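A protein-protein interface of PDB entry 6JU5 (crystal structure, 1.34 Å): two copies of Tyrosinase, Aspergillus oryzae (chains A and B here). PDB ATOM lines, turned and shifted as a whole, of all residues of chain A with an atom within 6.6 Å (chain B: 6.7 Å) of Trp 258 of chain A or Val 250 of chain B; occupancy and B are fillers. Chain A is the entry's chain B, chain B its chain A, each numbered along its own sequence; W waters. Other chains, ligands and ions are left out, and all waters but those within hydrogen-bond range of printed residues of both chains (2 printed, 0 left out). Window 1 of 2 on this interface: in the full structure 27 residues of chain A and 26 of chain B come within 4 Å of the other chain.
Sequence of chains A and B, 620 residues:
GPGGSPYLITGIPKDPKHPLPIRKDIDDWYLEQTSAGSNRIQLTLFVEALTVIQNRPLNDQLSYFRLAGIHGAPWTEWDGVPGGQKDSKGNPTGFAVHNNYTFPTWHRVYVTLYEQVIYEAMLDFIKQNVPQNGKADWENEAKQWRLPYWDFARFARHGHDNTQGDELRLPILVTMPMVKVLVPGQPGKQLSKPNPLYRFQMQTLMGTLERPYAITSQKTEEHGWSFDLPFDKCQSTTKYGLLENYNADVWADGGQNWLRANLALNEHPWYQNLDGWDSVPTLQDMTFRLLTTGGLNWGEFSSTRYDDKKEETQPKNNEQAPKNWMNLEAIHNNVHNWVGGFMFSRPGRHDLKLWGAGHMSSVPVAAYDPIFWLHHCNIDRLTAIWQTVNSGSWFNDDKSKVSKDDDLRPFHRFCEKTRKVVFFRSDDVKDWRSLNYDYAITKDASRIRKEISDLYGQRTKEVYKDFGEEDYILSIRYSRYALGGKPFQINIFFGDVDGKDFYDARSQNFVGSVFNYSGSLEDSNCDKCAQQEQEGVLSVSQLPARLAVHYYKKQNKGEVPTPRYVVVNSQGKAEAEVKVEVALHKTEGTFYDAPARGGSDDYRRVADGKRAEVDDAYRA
The backbone NH (N) of Asp 249 of chain B sits at hydrogen-bond distance from the side-chain amide oxygen (OD1) of Asn 247 of chain B, at 2.9 Å. OD1 of Asp 253 of chain B lies within hydrogen-bond range of N of Gly 255 of chain B. OE2 of Glu 167 of chain A is in salt-bridge range of NE of Arg 169 of chain A (2.8 Å). O of Trp 258 of chain A sits close to OD1 of Asn 262 of chain A (3.5 Å). The backbone carbonyl oxygen of Ile 172 of chain A lies within hydrogen-bond range of the side-chain hydroxyl of Thr 175 of chain A (2.7 Å).
Among the printed residues, pairs that only touch across the chains: Pro 177 of chain A with Asp 253 of chain B (3.1 Å), Arg 169 of chain A with Tyr 246 of chain B (3.3 Å), Thr 175 of chain A with Val 250 of chain B (3.5 Å), Leu 259 of chain A with Tyr 246 of chain B (3.5 Å), Trp 258 of chain A with Tyr 246 of chain B (3.6 Å), Glu 167 of chain A with Tyr 246 of chain B (3.7 Å), Trp 258 of chain A with Val 250 of chain B (3.7 Å), Ile 172 of chain A with Asn 247 of chain B (3.8 Å) and Met 176 of chain A with Asp 249 of chain B (3.9 Å).
Printed residues of chain B within 4 Å of Glu 167 of chain A: Tyr 246 (3.7 Å). Of the printed residues of chain B, Arg 169 of chain A touches Tyr 246. Of chain B, only Tyr 246 and Val 250 come within 4 Å of Trp 258 of chain A. Lys 233 of chain B touches none of the printed residues of chain A. Of the printed residues of chain A, Asp 249 of chain B touches Met 176 (3.9 Å). Val 250 of chain B touches just these residues of chain A: Thr 175 and Trp 258. The nearest printed residue of chain A that does not touch Asn 247 of chain B is Arg 169 of chain A (5.2 Å).
Printed residues of chain B that touch a printed residue of chain A: Tyr 246, Asn 247, Asp 249, Val 250 and Asp 253. Hydrophobic or aromatic side chains of chain B within 4 Å of the printed part of chain A: Tyr 246 and Val 250. Of the 22 printed residues of chain A, 8 touch a printed residue of chain B. Among the printed residues, no Asp or Glu carboxylate lies within 4 Å of a Lys or Arg side-chain nitrogen of the other chain.
1 position is printed for both chains. Of the 9 pairs that touch across the chains among the printed residues, none has its exchanged pair printed and touching as well.
Water W1 lies within hydrogen-bond range of OH of Tyr 246 of chain B, OE2 of Glu 167 of chain A and ND2 of Asn 262 of chain A. Water W2 lies within hydrogen-bond range of the backbone carbonyl oxygen of Thr 175 of chain A, the backbone carbonyl oxygen of Asp 253 of chain B and the indole nitrogen of Trp 258 of chain A.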
ATOM      1  N   GLU A 167     -14.764  21.944  -2.320  1.00  0.00           N
ATOM      2  CA  GLU A 167     -16.111  22.516  -2.418  1.00  0.00           C
ATOM      3  C   GLU A 167     -17.116  21.397  -2.649  1.00  0.00           C
ATOM      4  O   GLU A 167     -16.755  20.315  -3.146  1.00  0.00           O
ATOM      5  CB  GLU A 167     -16.204  23.591  -3.491  1.00  0.00           C
ATOM      6  CG  GLU A 167     -16.262  23.116  -4.915  1.00  0.00           C
ATOM      7  CD  GLU A 167     -16.501  24.203  -5.947  1.00  0.00           C
ATOM      8  OE1 GLU A 167     -16.633  25.397  -5.581  1.00  0.00           O
ATOM      9  OE2 GLU A 167     -16.565  23.862  -7.147  1.00  0.00           O
ATOM     10  N   ARG A 169     -20.317  19.858  -4.719  1.00  0.00           N
ATOM     11  CA  ARG A 169     -20.667  20.007  -6.132  1.00  0.00           C
ATOM     12  C   ARG A 169     -21.757  19.026  -6.522  1.00  0.00           C
ATOM     13  O   ARG A 169     -21.853  17.936  -5.958  1.00  0.00           O
ATOM     14  CB  ARG A 169     -19.466  19.652  -7.034  1.00  0.00           C
ATOM     15  CG  ARG A 169     -18.277  20.574  -6.952  1.00  0.00           C
ATOM     16  CD  ARG A 169     -17.213  20.183  -7.986  1.00  0.00           C
ATOM     17  NE  ARG A 169     -16.124  21.168  -7.960  1.00  0.00           N
ATOM     18  CZ  ARG A 169     -15.009  21.013  -8.670  1.00  0.00           C
ATOM     19  NH1 ARG A 169     -14.819  19.923  -9.404  1.00  0.00           N
ATOM     20  NH2 ARG A 169     -14.056  21.931  -8.648  1.00  0.00           N
ATOM     21  N   LEU A 170     -22.508  19.393  -7.548  1.00  0.00           N
ATOM     22  CA  LEU A 170     -23.331  18.453  -8.301  1.00  0.00           C
ATOM     23  C   LEU A 170     -22.491  17.292  -8.821  1.00  0.00           C
ATOM     24  O   LEU A 170     -21.305  17.485  -9.114  1.00  0.00           O
ATOM     25  CB  LEU A 170     -23.979  19.171  -9.489  1.00  0.00           C
ATOM     26  CG  LEU A 170     -25.107  20.153  -9.153  1.00  0.00           C
ATOM     27  CD1 LEU A 170     -25.555  20.880 -10.411  1.00  0.00           C
ATOM     28  CD2 LEU A 170     -26.268  19.424  -8.495  1.00  0.00           C
ATOM     29  N   ILE A 172     -20.485  14.808 -11.147  1.00  0.00           N
ATOM     30  CA  ILE A 172     -19.838  14.957 -12.448  1.00  0.00           C
ATOM     31  C   ILE A 172     -20.795  14.616 -13.575  1.00  0.00           C
ATOM     32  O   ILE A 172     -20.955  15.372 -14.529  1.00  0.00           O
ATOM     33  CB  ILE A 172     -18.584  14.064 -12.542  1.00  0.00           C
ATOM     34  CG1 ILE A 172     -17.543  14.391 -11.466  1.00  0.00           C
ATOM     35  CG2 ILE A 172     -17.931  14.128 -13.921  1.00  0.00           C
ATOM     36  CD1 ILE A 172     -16.526  13.279 -11.273  1.00  0.00           C
ATOM     37  N   LEU A 173     -21.427  13.442 -13.448  1.00  0.00           N
ATOM     38  CA  LEU A 173     -22.288  12.947 -14.518  1.00  0.00           C
ATOM     39  C   LEU A 173     -23.460  13.867 -14.812  1.00  0.00           C
ATOM     40  O   LEU A 173     -23.878  13.942 -15.973  1.00  0.00           O
ATOM     41  CB  LEU A 173     -22.909  11.609 -14.112  1.00  0.00           C
ATOM     42  CG  LEU A 173     -22.345  10.406 -14.822  1.00  0.00           C
ATOM     43  CD1 LEU A 173     -23.097   9.155 -14.401  1.00  0.00           C
ATOM     44  CD2 LEU A 173     -22.421  10.555 -16.341  1.00  0.00           C
ATOM     45  N   VAL A 174     -24.015  14.483 -13.771  1.00  0.00           N
ATOM     46  CA  VAL A 174     -25.156  15.390 -13.994  1.00  0.00           C
ATOM     47  C   VAL A 174     -24.766  16.623 -14.793  1.00  0.00           C
ATOM     48  O   VAL A 174     -25.588  17.313 -15.415  1.00  0.00           O
ATOM     49  CB  VAL A 174     -25.730  15.707 -12.591  1.00  0.00           C
ATOM     50  CG1 VAL A 174     -26.537  16.981 -12.557  1.00  0.00           C
ATOM     51  CG2 VAL A 174     -26.578  14.526 -12.102  1.00  0.00           C
ATOM     52  N   THR A 175     -23.453  16.926 -14.862  1.00  0.00           N
ATOM     53  CA  THR A 175     -22.978  18.122 -15.541  1.00  0.00           C
ATOM     54  C   THR A 175     -22.515  17.861 -16.965  1.00  0.00           C
ATOM     55  O   THR A 175     -22.009  18.777 -17.628  1.00  0.00           O
ATOM     56  CB  THR A 175     -21.854  18.845 -14.754  1.00  0.00           C
ATOM     57  OG1 THR A 175     -20.649  18.073 -14.765  1.00  0.00           O
ATOM     58  CG2 THR A 175     -22.304  19.067 -13.312  1.00  0.00           C
ATOM     59  N   MET A 176     -22.693  16.640 -17.454  1.00  0.00           N
ATOM     60  CA  MET A 176     -22.235  16.220 -18.787  1.00  0.00           C
ATOM     61  C   MET A 176     -23.410  16.071 -19.739  1.00  0.00           C
ATOM     62  O   MET A 176     -24.273  15.198 -19.538  1.00  0.00           O
ATOM     63  CB  MET A 176     -21.505  14.882 -18.657  1.00  0.00           C
ATOM     64  CG  MET A 176     -20.158  14.979 -17.944  1.00  0.00           C
ATOM     65  SD  MET A 176     -19.539  13.330 -17.498  1.00  0.00           S
ATOM     66  CE  MET A 176     -19.653  12.516 -19.095  1.00  0.00           C
ATOM     67  N   PRO A 177     -23.521  16.885 -20.787  1.00  0.00           N
ATOM     68  CA  PRO A 177     -24.621  16.691 -21.734  1.00  0.00           C
ATOM     69  C   PRO A 177     -24.631  15.339 -22.452  1.00  0.00           C
ATOM     70  O   PRO A 177     -25.719  14.856 -22.789  1.00  0.00           O
ATOM     71  CB  PRO A 177     -24.382  17.816 -22.762  1.00  0.00           C
ATOM     72  CG  PRO A 177     -23.706  18.893 -21.943  1.00  0.00           C
ATOM     73  CD  PRO A 177     -22.762  18.126 -21.048  1.00  0.00           C
ATOM     74  N   TYR A 198     -28.617  14.269 -17.337  1.00  0.00           N
ATOM     75  CA  TYR A 198     -28.377  15.709 -17.488  1.00  0.00           C
ATOM     76  C   TYR A 198     -29.672  16.508 -17.416  1.00  0.00           C
ATOM     77  O   TYR A 198     -29.684  17.620 -16.906  1.00  0.00           O
ATOM     78  CB  TYR A 198     -27.711  15.948 -18.827  1.00  0.00           C
ATOM     79  CG  TYR A 198     -27.273  17.344 -19.188  1.00  0.00           C
ATOM     80  CD1 TYR A 198     -26.217  17.970 -18.531  1.00  0.00           C
ATOM     81  CD2 TYR A 198     -27.909  17.993 -20.239  1.00  0.00           C
ATOM     82  CE1 TYR A 198     -25.818  19.260 -18.896  1.00  0.00           C
ATOM     83  CE2 TYR A 198     -27.513  19.264 -20.600  1.00  0.00           C
ATOM     84  CZ  TYR A 198     -26.478  19.891 -19.930  1.00  0.00           C
ATOM     85  OH  TYR A 198     -26.104  21.148 -20.353  1.00  0.00           O
ATOM     86  N   LYS A 239     -32.067  23.890 -14.509  1.00  0.00           N
ATOM     87  CA  LYS A 239     -31.520  24.407 -13.247  1.00  0.00           C
ATOM     88  C   LYS A 239     -31.184  25.894 -13.448  1.00  0.00           C
ATOM     89  O   LYS A 239     -30.325  26.185 -14.285  1.00  0.00           O
ATOM     90  CB  LYS A 239     -30.268  23.626 -12.835  1.00  0.00           C
ATOM     91  CG  LYS A 239     -30.519  22.126 -12.659  1.00  0.00           C
ATOM     92  CD  LYS A 239     -29.202  21.380 -12.497  1.00  0.00           C
ATOM     93  CE  LYS A 239     -29.367  19.884 -12.310  1.00  0.00           C
ATOM     94  NZ  LYS A 239     -30.051  19.309 -13.508  1.00  0.00           N
ATOM     95  N   TYR A 240     -31.865  26.795 -12.743  1.00  0.00           N
ATOM     96  CA  TYR A 240     -31.669  28.242 -12.825  1.00  0.00           C
ATOM     97  C   TYR A 240     -31.982  28.791 -14.217  1.00  0.00           C
ATOM     98  O   TYR A 240     -31.602  29.922 -14.529  1.00  0.00           O
ATOM     99  CB  TYR A 240     -30.258  28.690 -12.391  1.00  0.00           C
ATOM    100  CG  TYR A 240     -30.020  28.444 -10.919  1.00  0.00           C
ATOM    101  CD1 TYR A 240     -29.627  27.194 -10.458  1.00  0.00           C
ATOM    102  CD2 TYR A 240     -30.211  29.465  -9.981  1.00  0.00           C
ATOM    103  CE1 TYR A 240     -29.426  26.966  -9.116  1.00  0.00           C
ATOM    104  CE2 TYR A 240     -30.003  29.226  -8.628  1.00  0.00           C
ATOM    105  CZ  TYR A 240     -29.609  27.978  -8.196  1.00  0.00           C
ATOM    106  OH  TYR A 240     -29.409  27.776  -6.849  1.00  0.00           O
ATOM    107  N   GLY A 255     -31.723  25.216 -19.905  1.00  0.00           N
ATOM    108  CA  GLY A 255     -30.360  24.772 -19.692  1.00  0.00           C
ATOM    109  C   GLY A 255     -30.079  24.309 -18.276  1.00  0.00           C
ATOM    110  O   GLY A 255     -30.922  24.360 -17.377  1.00  0.00           O
ATOM    111  N   GLN A 256     -28.855  23.826 -18.090  1.00  0.00           N
ATOM    112  CA  GLN A 256     -28.405  23.303 -16.801  1.00  0.00           C
ATOM    113  C   GLN A 256     -27.285  24.192 -16.274  1.00  0.00           C
ATOM    114  O   GLN A 256     -26.121  23.979 -16.633  1.00  0.00           O
ATOM    115  CB  GLN A 256     -27.926  21.862 -16.945  1.00  0.00           C
ATOM    116  CG  GLN A 256     -28.877  21.015 -17.771  1.00  0.00           C
ATOM    117  CD  GLN A 256     -30.304  21.020 -17.264  1.00  0.00           C
ATOM    118  OE1 GLN A 256     -30.594  20.996 -16.071  1.00  0.00           O
ATOM    119  NE2 GLN A 256     -31.233  21.044 -18.223  1.00  0.00           N
ATOM    120  N   ASN A 257     -27.657  25.183 -15.461  1.00  0.00           N
ATOM    121  CA  ASN A 257     -26.614  26.070 -14.946  1.00  0.00           C
ATOM    122  C   ASN A 257     -26.003  25.456 -13.684  1.00  0.00           C
ATOM    123  O   ASN A 257     -26.215  25.889 -12.554  1.00  0.00           O
ATOM    124  CB  ASN A 257     -27.158  27.466 -14.660  1.00  0.00           C
ATOM    125  CG  ASN A 257     -26.068  28.513 -14.554  1.00  0.00           C
ATOM    126  OD1 ASN A 257     -24.896  28.228 -14.308  1.00  0.00           O
ATOM    127  ND2 ASN A 257     -26.480  29.764 -14.758  1.00  0.00           N
ATOM    128  N   TRP A 258     -25.206  24.420 -13.942  1.00  0.00           N
ATOM    129  CA  TRP A 258     -24.630  23.619 -12.874  1.00  0.00           C
ATOM    130  C   TRP A 258     -23.587  24.368 -12.069  1.00  0.00           C
ATOM    131  O   TRP A 258     -23.455  24.160 -10.860  1.00  0.00           O
ATOM    132  CB  TRP A 258     -24.108  22.290 -13.428  1.00  0.00           C
ATOM    133  CG  TRP A 258     -22.972  22.361 -14.394  1.00  0.00           C
ATOM    134  CD1 TRP A 258     -23.018  22.276 -15.763  1.00  0.00           C
ATOM    135  CD2 TRP A 258     -21.588  22.518 -14.051  1.00  0.00           C
ATOM    136  NE1 TRP A 258     -21.742  22.381 -16.276  1.00  0.00           N
ATOM    137  CE2 TRP A 258     -20.851  22.532 -15.246  1.00  0.00           C
ATOM    138  CE3 TRP A 258     -20.895  22.653 -12.834  1.00  0.00           C
ATOM    139  CZ2 TRP A 258     -19.461  22.676 -15.287  1.00  0.00           C
ATOM    140  CZ3 TRP A 258     -19.521  22.797 -12.864  1.00  0.00           C
ATOM    141  CH2 TRP A 258     -18.824  22.804 -14.081  1.00  0.00           C
ATOM    142  N   LEU A 259     -22.902  25.331 -12.700  1.00  0.00           N
ATOM    143  CA  LEU A 259     -21.986  26.186 -11.945  1.00  0.00           C
ATOM    144  C   LEU A 259     -22.744  27.059 -10.941  1.00  0.00           C
ATOM    145  O   LEU A 259     -22.287  27.253  -9.799  1.00  0.00           O
ATOM    146  CB  LEU A 259     -21.206  27.064 -12.911  1.00  0.00           C
ATOM    147  CG  LEU A 259     -19.802  27.510 -12.577  1.00  0.00           C
ATOM    148  CD1 LEU A 259     -18.865  26.361 -12.231  1.00  0.00           C
ATOM    149  CD2 LEU A 259     -19.259  28.321 -13.750  1.00  0.00           C
ATOM    150  N   ARG A 260     -23.915  27.545 -11.354  1.00  0.00           N
ATOM    151  CA  ARG A 260     -24.712  28.355 -10.415  1.00  0.00           C
ATOM    152  C   ARG A 260     -25.269  27.514  -9.277  1.00  0.00           C
ATOM    153  O   ARG A 260     -25.305  27.922  -8.101  1.00  0.00           O
ATOM    154  CB  ARG A 260     -25.818  29.081 -11.184  1.00  0.00           C
ATOM    155  CG  ARG A 260     -26.754  29.858 -10.242  1.00  0.00           C
ATOM    156  CD  ARG A 260     -26.012  31.023  -9.620  1.00  0.00           C
ATOM    157  NE  ARG A 260     -26.822  31.808  -8.697  1.00  0.00           N
ATOM    158  CZ  ARG A 260     -26.903  31.603  -7.391  1.00  0.00           C
ATOM    159  NH1 ARG A 260     -26.214  30.592  -6.856  1.00  0.00           N
ATOM    160  NH2 ARG A 260     -27.665  32.410  -6.663  1.00  0.00           N
ATOM    161  N   ALA A 261     -25.689  26.292  -9.582  1.00  0.00           N
ATOM    162  CA  ALA A 261     -26.162  25.370  -8.551  1.00  0.00           C
ATOM    163  C   ALA A 261     -25.036  25.035  -7.580  1.00  0.00           C
ATOM    164  O   ALA A 261     -25.252  25.034  -6.367  1.00  0.00           O
ATOM    165  CB  ALA A 261     -26.705  24.101  -9.198  1.00  0.00           C
ATOM    166  N   ASN A 262     -23.823  24.798  -8.087  1.00  0.00           N
ATOM    167  CA  ASN A 262     -22.688  24.536  -7.195  1.00  0.00           C
ATOM    168  C   ASN A 262     -22.463  25.739  -6.279  1.00  0.00           C
ATOM    169  O   ASN A 262     -22.166  25.574  -5.095  1.00  0.00           O
ATOM    170  CB  ASN A 262     -21.430  24.244  -7.997  1.00  0.00           C
ATOM    171  CG  ASN A 262     -21.394  22.850  -8.585  1.00  0.00           C
ATOM    172  OD1 ASN A 262     -22.302  22.053  -8.370  1.00  0.00           O
ATOM    173  ND2 ASN A 262     -20.324  22.538  -9.308  1.00  0.00           N
ATOM    174  N   LEU A 263     -22.589  26.953  -6.801  1.00  0.00           N
ATOM    175  CA  LEU A 263     -22.369  28.134  -5.961  1.00  0.00           C
ATOM    176  C   LEU A 263     -23.369  28.130  -4.816  1.00  0.00           C
ATOM    177  O   LEU A 263     -23.036  28.349  -3.656  1.00  0.00           O
ATOM    178  CB  LEU A 263     -22.510  29.418  -6.787  1.00  0.00           C
ATOM    179  CG  LEU A 263     -22.442  30.735  -6.009  1.00  0.00           C
ATOM    180  CD1 LEU A 263     -21.092  30.891  -5.319  1.00  0.00           C
ATOM    181  CD2 LEU A 263     -22.677  31.900  -6.957  1.00  0.00           C
ATOM    182  N   LEU A 265     -24.986  25.597  -3.530  1.00  0.00           N
ATOM    183  CA  LEU A 265     -24.729  24.476  -2.616  1.00  0.00           C
ATOM    184  C   LEU A 265     -23.602  24.774  -1.636  1.00  0.00           C
ATOM    185  O   LEU A 265     -23.571  24.142  -0.578  1.00  0.00           O
ATOM    186  CB  LEU A 265     -24.398  23.200  -3.403  1.00  0.00           C
ATOM    187  CG  LEU A 265     -25.575  22.633  -4.200  1.00  0.00           C
ATOM    188  CD1 LEU A 265     -25.070  21.753  -5.339  1.00  0.00           C
ATOM    189  CD2 LEU A 265     -26.527  21.869  -3.287  1.00  0.00           C
ATOM    190  N   LYS B 233     -10.332  18.325 -26.537  1.00  0.00           N
ATOM    191  CA  LYS B 233     -11.129  17.475 -25.659  1.00  0.00           C
ATOM    192  C   LYS B 233     -12.609  17.848 -25.734  1.00  0.00           C
ATOM    193  O   LYS B 233     -13.427  17.418 -24.913  1.00  0.00           O
ATOM    194  CB  LYS B 233     -10.629  17.525 -24.216  1.00  0.00           C
ATOM    195  CG  LYS B 233      -9.153  16.945 -24.120  1.00  0.00           C
ATOM    196  N   GLY B 241     -17.579  27.363 -21.085  1.00  0.00           N
ATOM    197  CA  GLY B 241     -17.809  26.032 -20.519  1.00  0.00           C
ATOM    198  C   GLY B 241     -16.530  25.372 -20.034  1.00  0.00           C
ATOM    199  O   GLY B 241     -16.576  24.376 -19.294  1.00  0.00           O
ATOM    200  N   LEU B 242     -15.364  25.860 -20.442  1.00  0.00           N
ATOM    201  CA  LEU B 242     -14.096  25.196 -20.121  1.00  0.00           C
ATOM    202  C   LEU B 242     -13.450  25.880 -18.923  1.00  0.00           C
ATOM    203  O   LEU B 242     -12.972  27.016 -19.029  1.00  0.00           O
ATOM    204  CB  LEU B 242     -13.145  25.204 -21.327  1.00  0.00           C
ATOM    205  CG  LEU B 242     -13.747  24.674 -22.635  1.00  0.00           C
ATOM    206  CD1 LEU B 242     -12.754  24.772 -23.788  1.00  0.00           C
ATOM    207  CD2 LEU B 242     -14.288  23.268 -22.450  1.00  0.00           C
ATOM    208  N   LEU B 243     -13.433  25.176 -17.801  1.00  0.00           N
ATOM    209  CA  LEU B 243     -12.818  25.624 -16.557  1.00  0.00           C
ATOM    210  C   LEU B 243     -11.868  24.537 -16.028  1.00  0.00           C
ATOM    211  O   LEU B 243     -12.222  23.348 -16.077  1.00  0.00           O
ATOM    212  CB  LEU B 243     -13.863  25.903 -15.466  1.00  0.00           C
ATOM    213  CG  LEU B 243     -14.679  27.201 -15.627  1.00  0.00           C
ATOM    214  CD1 LEU B 243     -15.867  26.997 -16.554  1.00  0.00           C
ATOM    215  CD2 LEU B 243     -15.160  27.710 -14.272  1.00  0.00           C
ATOM    216  N   TYR B 246     -12.288  20.820 -13.116  1.00  0.00           N
ATOM    217  CA  TYR B 246     -13.444  19.940 -13.286  1.00  0.00           C
ATOM    218  C   TYR B 246     -12.989  18.729 -14.079  1.00  0.00           C
ATOM    219  O   TYR B 246     -11.950  18.786 -14.755  1.00  0.00           O
ATOM    220  CB  TYR B 246     -14.623  20.649 -14.016  1.00  0.00           C
ATOM    221  CG  TYR B 246     -15.042  21.794 -13.109  1.00  0.00           C
ATOM    222  CD1 TYR B 246     -15.975  21.589 -12.089  1.00  0.00           C
ATOM    223  CD2 TYR B 246     -14.455  23.043 -13.268  1.00  0.00           C
ATOM    224  CE1 TYR B 246     -16.328  22.657 -11.264  1.00  0.00           C
ATOM    225  CE2 TYR B 246     -14.799  24.087 -12.429  1.00  0.00           C
ATOM    226  CZ  TYR B 246     -15.725  23.886 -11.440  1.00  0.00           C
ATOM    227  OH  TYR B 246     -16.041  24.950 -10.629  1.00  0.00           O
ATOM    228  N   ASN B 247     -13.762  17.646 -14.010  1.00  0.00           N
ATOM    229  CA  ASN B 247     -13.378  16.436 -14.735  1.00  0.00           C
ATOM    230  C   ASN B 247     -13.295  16.731 -16.227  1.00  0.00           C
ATOM    231  O   ASN B 247     -14.120  17.457 -16.785  1.00  0.00           O
ATOM    232  CB  ASN B 247     -14.422  15.354 -14.433  1.00  0.00           C
ATOM    233  CG  ASN B 247     -13.942  14.006 -14.943  1.00  0.00           C
ATOM    234  OD1 ASN B 247     -14.073  13.728 -16.136  1.00  0.00           O
ATOM    235  ND2 ASN B 247     -13.340  13.263 -14.031  1.00  0.00           N
ATOM    236  N   ALA B 248     -12.294  16.177 -16.891  1.00  0.00           N
ATOM    237  CA  ALA B 248     -12.079  16.465 -18.304  1.00  0.00           C
ATOM    238  C   ALA B 248     -13.272  16.074 -19.161  1.00  0.00           C
ATOM    239  O   ALA B 248     -13.470  16.609 -20.249  1.00  0.00           O
ATOM    240  CB  ALA B 248     -10.833  15.713 -18.751  1.00  0.00           C
ATOM    241  N   ASP B 249     -14.072  15.115 -18.699  1.00  0.00           N
ATOM    242  CA  ASP B 249     -15.255  14.714 -19.449  1.00  0.00           C
ATOM    243  C   ASP B 249     -16.302  15.821 -19.495  1.00  0.00           C
ATOM    244  O   ASP B 249     -17.156  15.807 -20.378  1.00  0.00           O
ATOM    245  CB  ASP B 249     -15.893  13.450 -18.867  1.00  0.00           C
ATOM    246  CG  ASP B 249     -15.000  12.236 -19.072  1.00  0.00           C
ATOM    247  OD1 ASP B 249     -14.148  12.275 -19.987  1.00  0.00           O
ATOM    248  OD2 ASP B 249     -15.175  11.252 -18.323  1.00  0.00           O
ATOM    249  N   VAL B 250     -16.226  16.783 -18.573  1.00  0.00           N
ATOM    250  CA  VAL B 250     -17.117  17.950 -18.642  1.00  0.00           C
ATOM    251  C   VAL B 250     -16.770  18.810 -19.853  1.00  0.00           C
ATOM    252  O   VAL B 250     -17.655  19.437 -20.445  1.00  0.00           O
ATOM    253  CB  VAL B 250     -17.028  18.742 -17.333  1.00  0.00           C
ATOM    254  CG1 VAL B 250     -17.918  19.972 -17.353  1.00  0.00           C
ATOM    255  CG2 VAL B 250     -17.439  17.852 -16.158  1.00  0.00           C
ATOM    256  N   TRP B 251     -15.508  18.806 -20.275  1.00  0.00           N
ATOM    257  CA  TRP B 251     -15.090  19.632 -21.404  1.00  0.00           C
ATOM    258  C   TRP B 251     -15.610  19.102 -22.724  1.00  0.00           C
ATOM    259  O   TRP B 251     -15.588  19.823 -23.744  1.00  0.00           O
ATOM    260  CB  TRP B 251     -13.562  19.748 -21.471  1.00  0.00           C
ATOM    261  CG  TRP B 251     -12.984  20.261 -20.181  1.00  0.00           C
ATOM    262  CD1 TRP B 251     -13.564  21.091 -19.260  1.00  0.00           C
ATOM    263  CD2 TRP B 251     -11.677  19.955 -19.684  1.00  0.00           C
ATOM    264  NE1 TRP B 251     -12.700  21.316 -18.216  1.00  0.00           N
ATOM    265  CE2 TRP B 251     -11.526  20.627 -18.456  1.00  0.00           C
ATOM    266  CE3 TRP B 251     -10.615  19.181 -20.164  1.00  0.00           C
ATOM    267  CZ2 TRP B 251     -10.356  20.534 -17.708  1.00  0.00           C
ATOM    268  CZ3 TRP B 251      -9.452  19.096 -19.403  1.00  0.00           C
ATOM    269  CH2 TRP B 251      -9.331  19.773 -18.183  1.00  0.00           C
ATOM    270  N   ALA B 252     -16.035  17.842 -22.765  1.00  0.00           N
ATOM    271  CA  ALA B 252     -16.572  17.331 -24.034  1.00  0.00           C
ATOM    272  C   ALA B 252     -17.689  18.238 -24.537  1.00  0.00           C
ATOM    273  O   ALA B 252     -17.770  18.501 -25.737  1.00  0.00           O
ATOM    274  CB  ALA B 252     -17.065  15.902 -23.875  1.00  0.00           C
ATOM    275  N   ASP B 253     -18.549  18.710 -23.649  1.00  0.00           N
ATOM    276  CA  ASP B 253     -19.595  19.684 -23.971  1.00  0.00           C
ATOM    277  C   ASP B 253     -19.802  20.555 -22.723  1.00  0.00           C
ATOM    278  O   ASP B 253     -20.501  20.127 -21.804  1.00  0.00           O
ATOM    279  CB  ASP B 253     -20.916  19.046 -24.375  1.00  0.00           C
ATOM    280  CG  ASP B 253     -21.946  20.062 -24.872  1.00  0.00           C
ATOM    281  OD1 ASP B 253     -21.870  21.274 -24.539  1.00  0.00           O
ATOM    282  OD2 ASP B 253     -22.896  19.649 -25.578  1.00  0.00           O
ATOM    283  N   GLY B 254     -19.129  21.697 -22.725  1.00  0.00           N
ATOM    284  CA  GLY B 254     -19.155  22.584 -21.568  1.00  0.00           C
ATOM    285  C   GLY B 254     -20.424  23.410 -21.469  1.00  0.00           C
ATOM    286  O   GLY B 254     -20.577  24.169 -20.501  1.00  0.00           O
ATOM    287  N   GLY B 255     -21.338  23.278 -22.426  1.00  0.00           N
ATOM    288  CA  GLY B 255     -22.614  23.980 -22.361  1.00  0.00           C
ATOM    289  C   GLY B 255     -22.514  25.372 -22.963  1.00  0.00           C
ATOM    290  O   GLY B 255     -21.466  25.819 -23.415  1.00  0.00           O
HETATM  291  O   HOH W   1     -18.230  24.787  -9.135  1.00  0.00           O
HETATM  292  O   HOH W   2     -21.415  20.998 -19.192  1.00  0.00           O
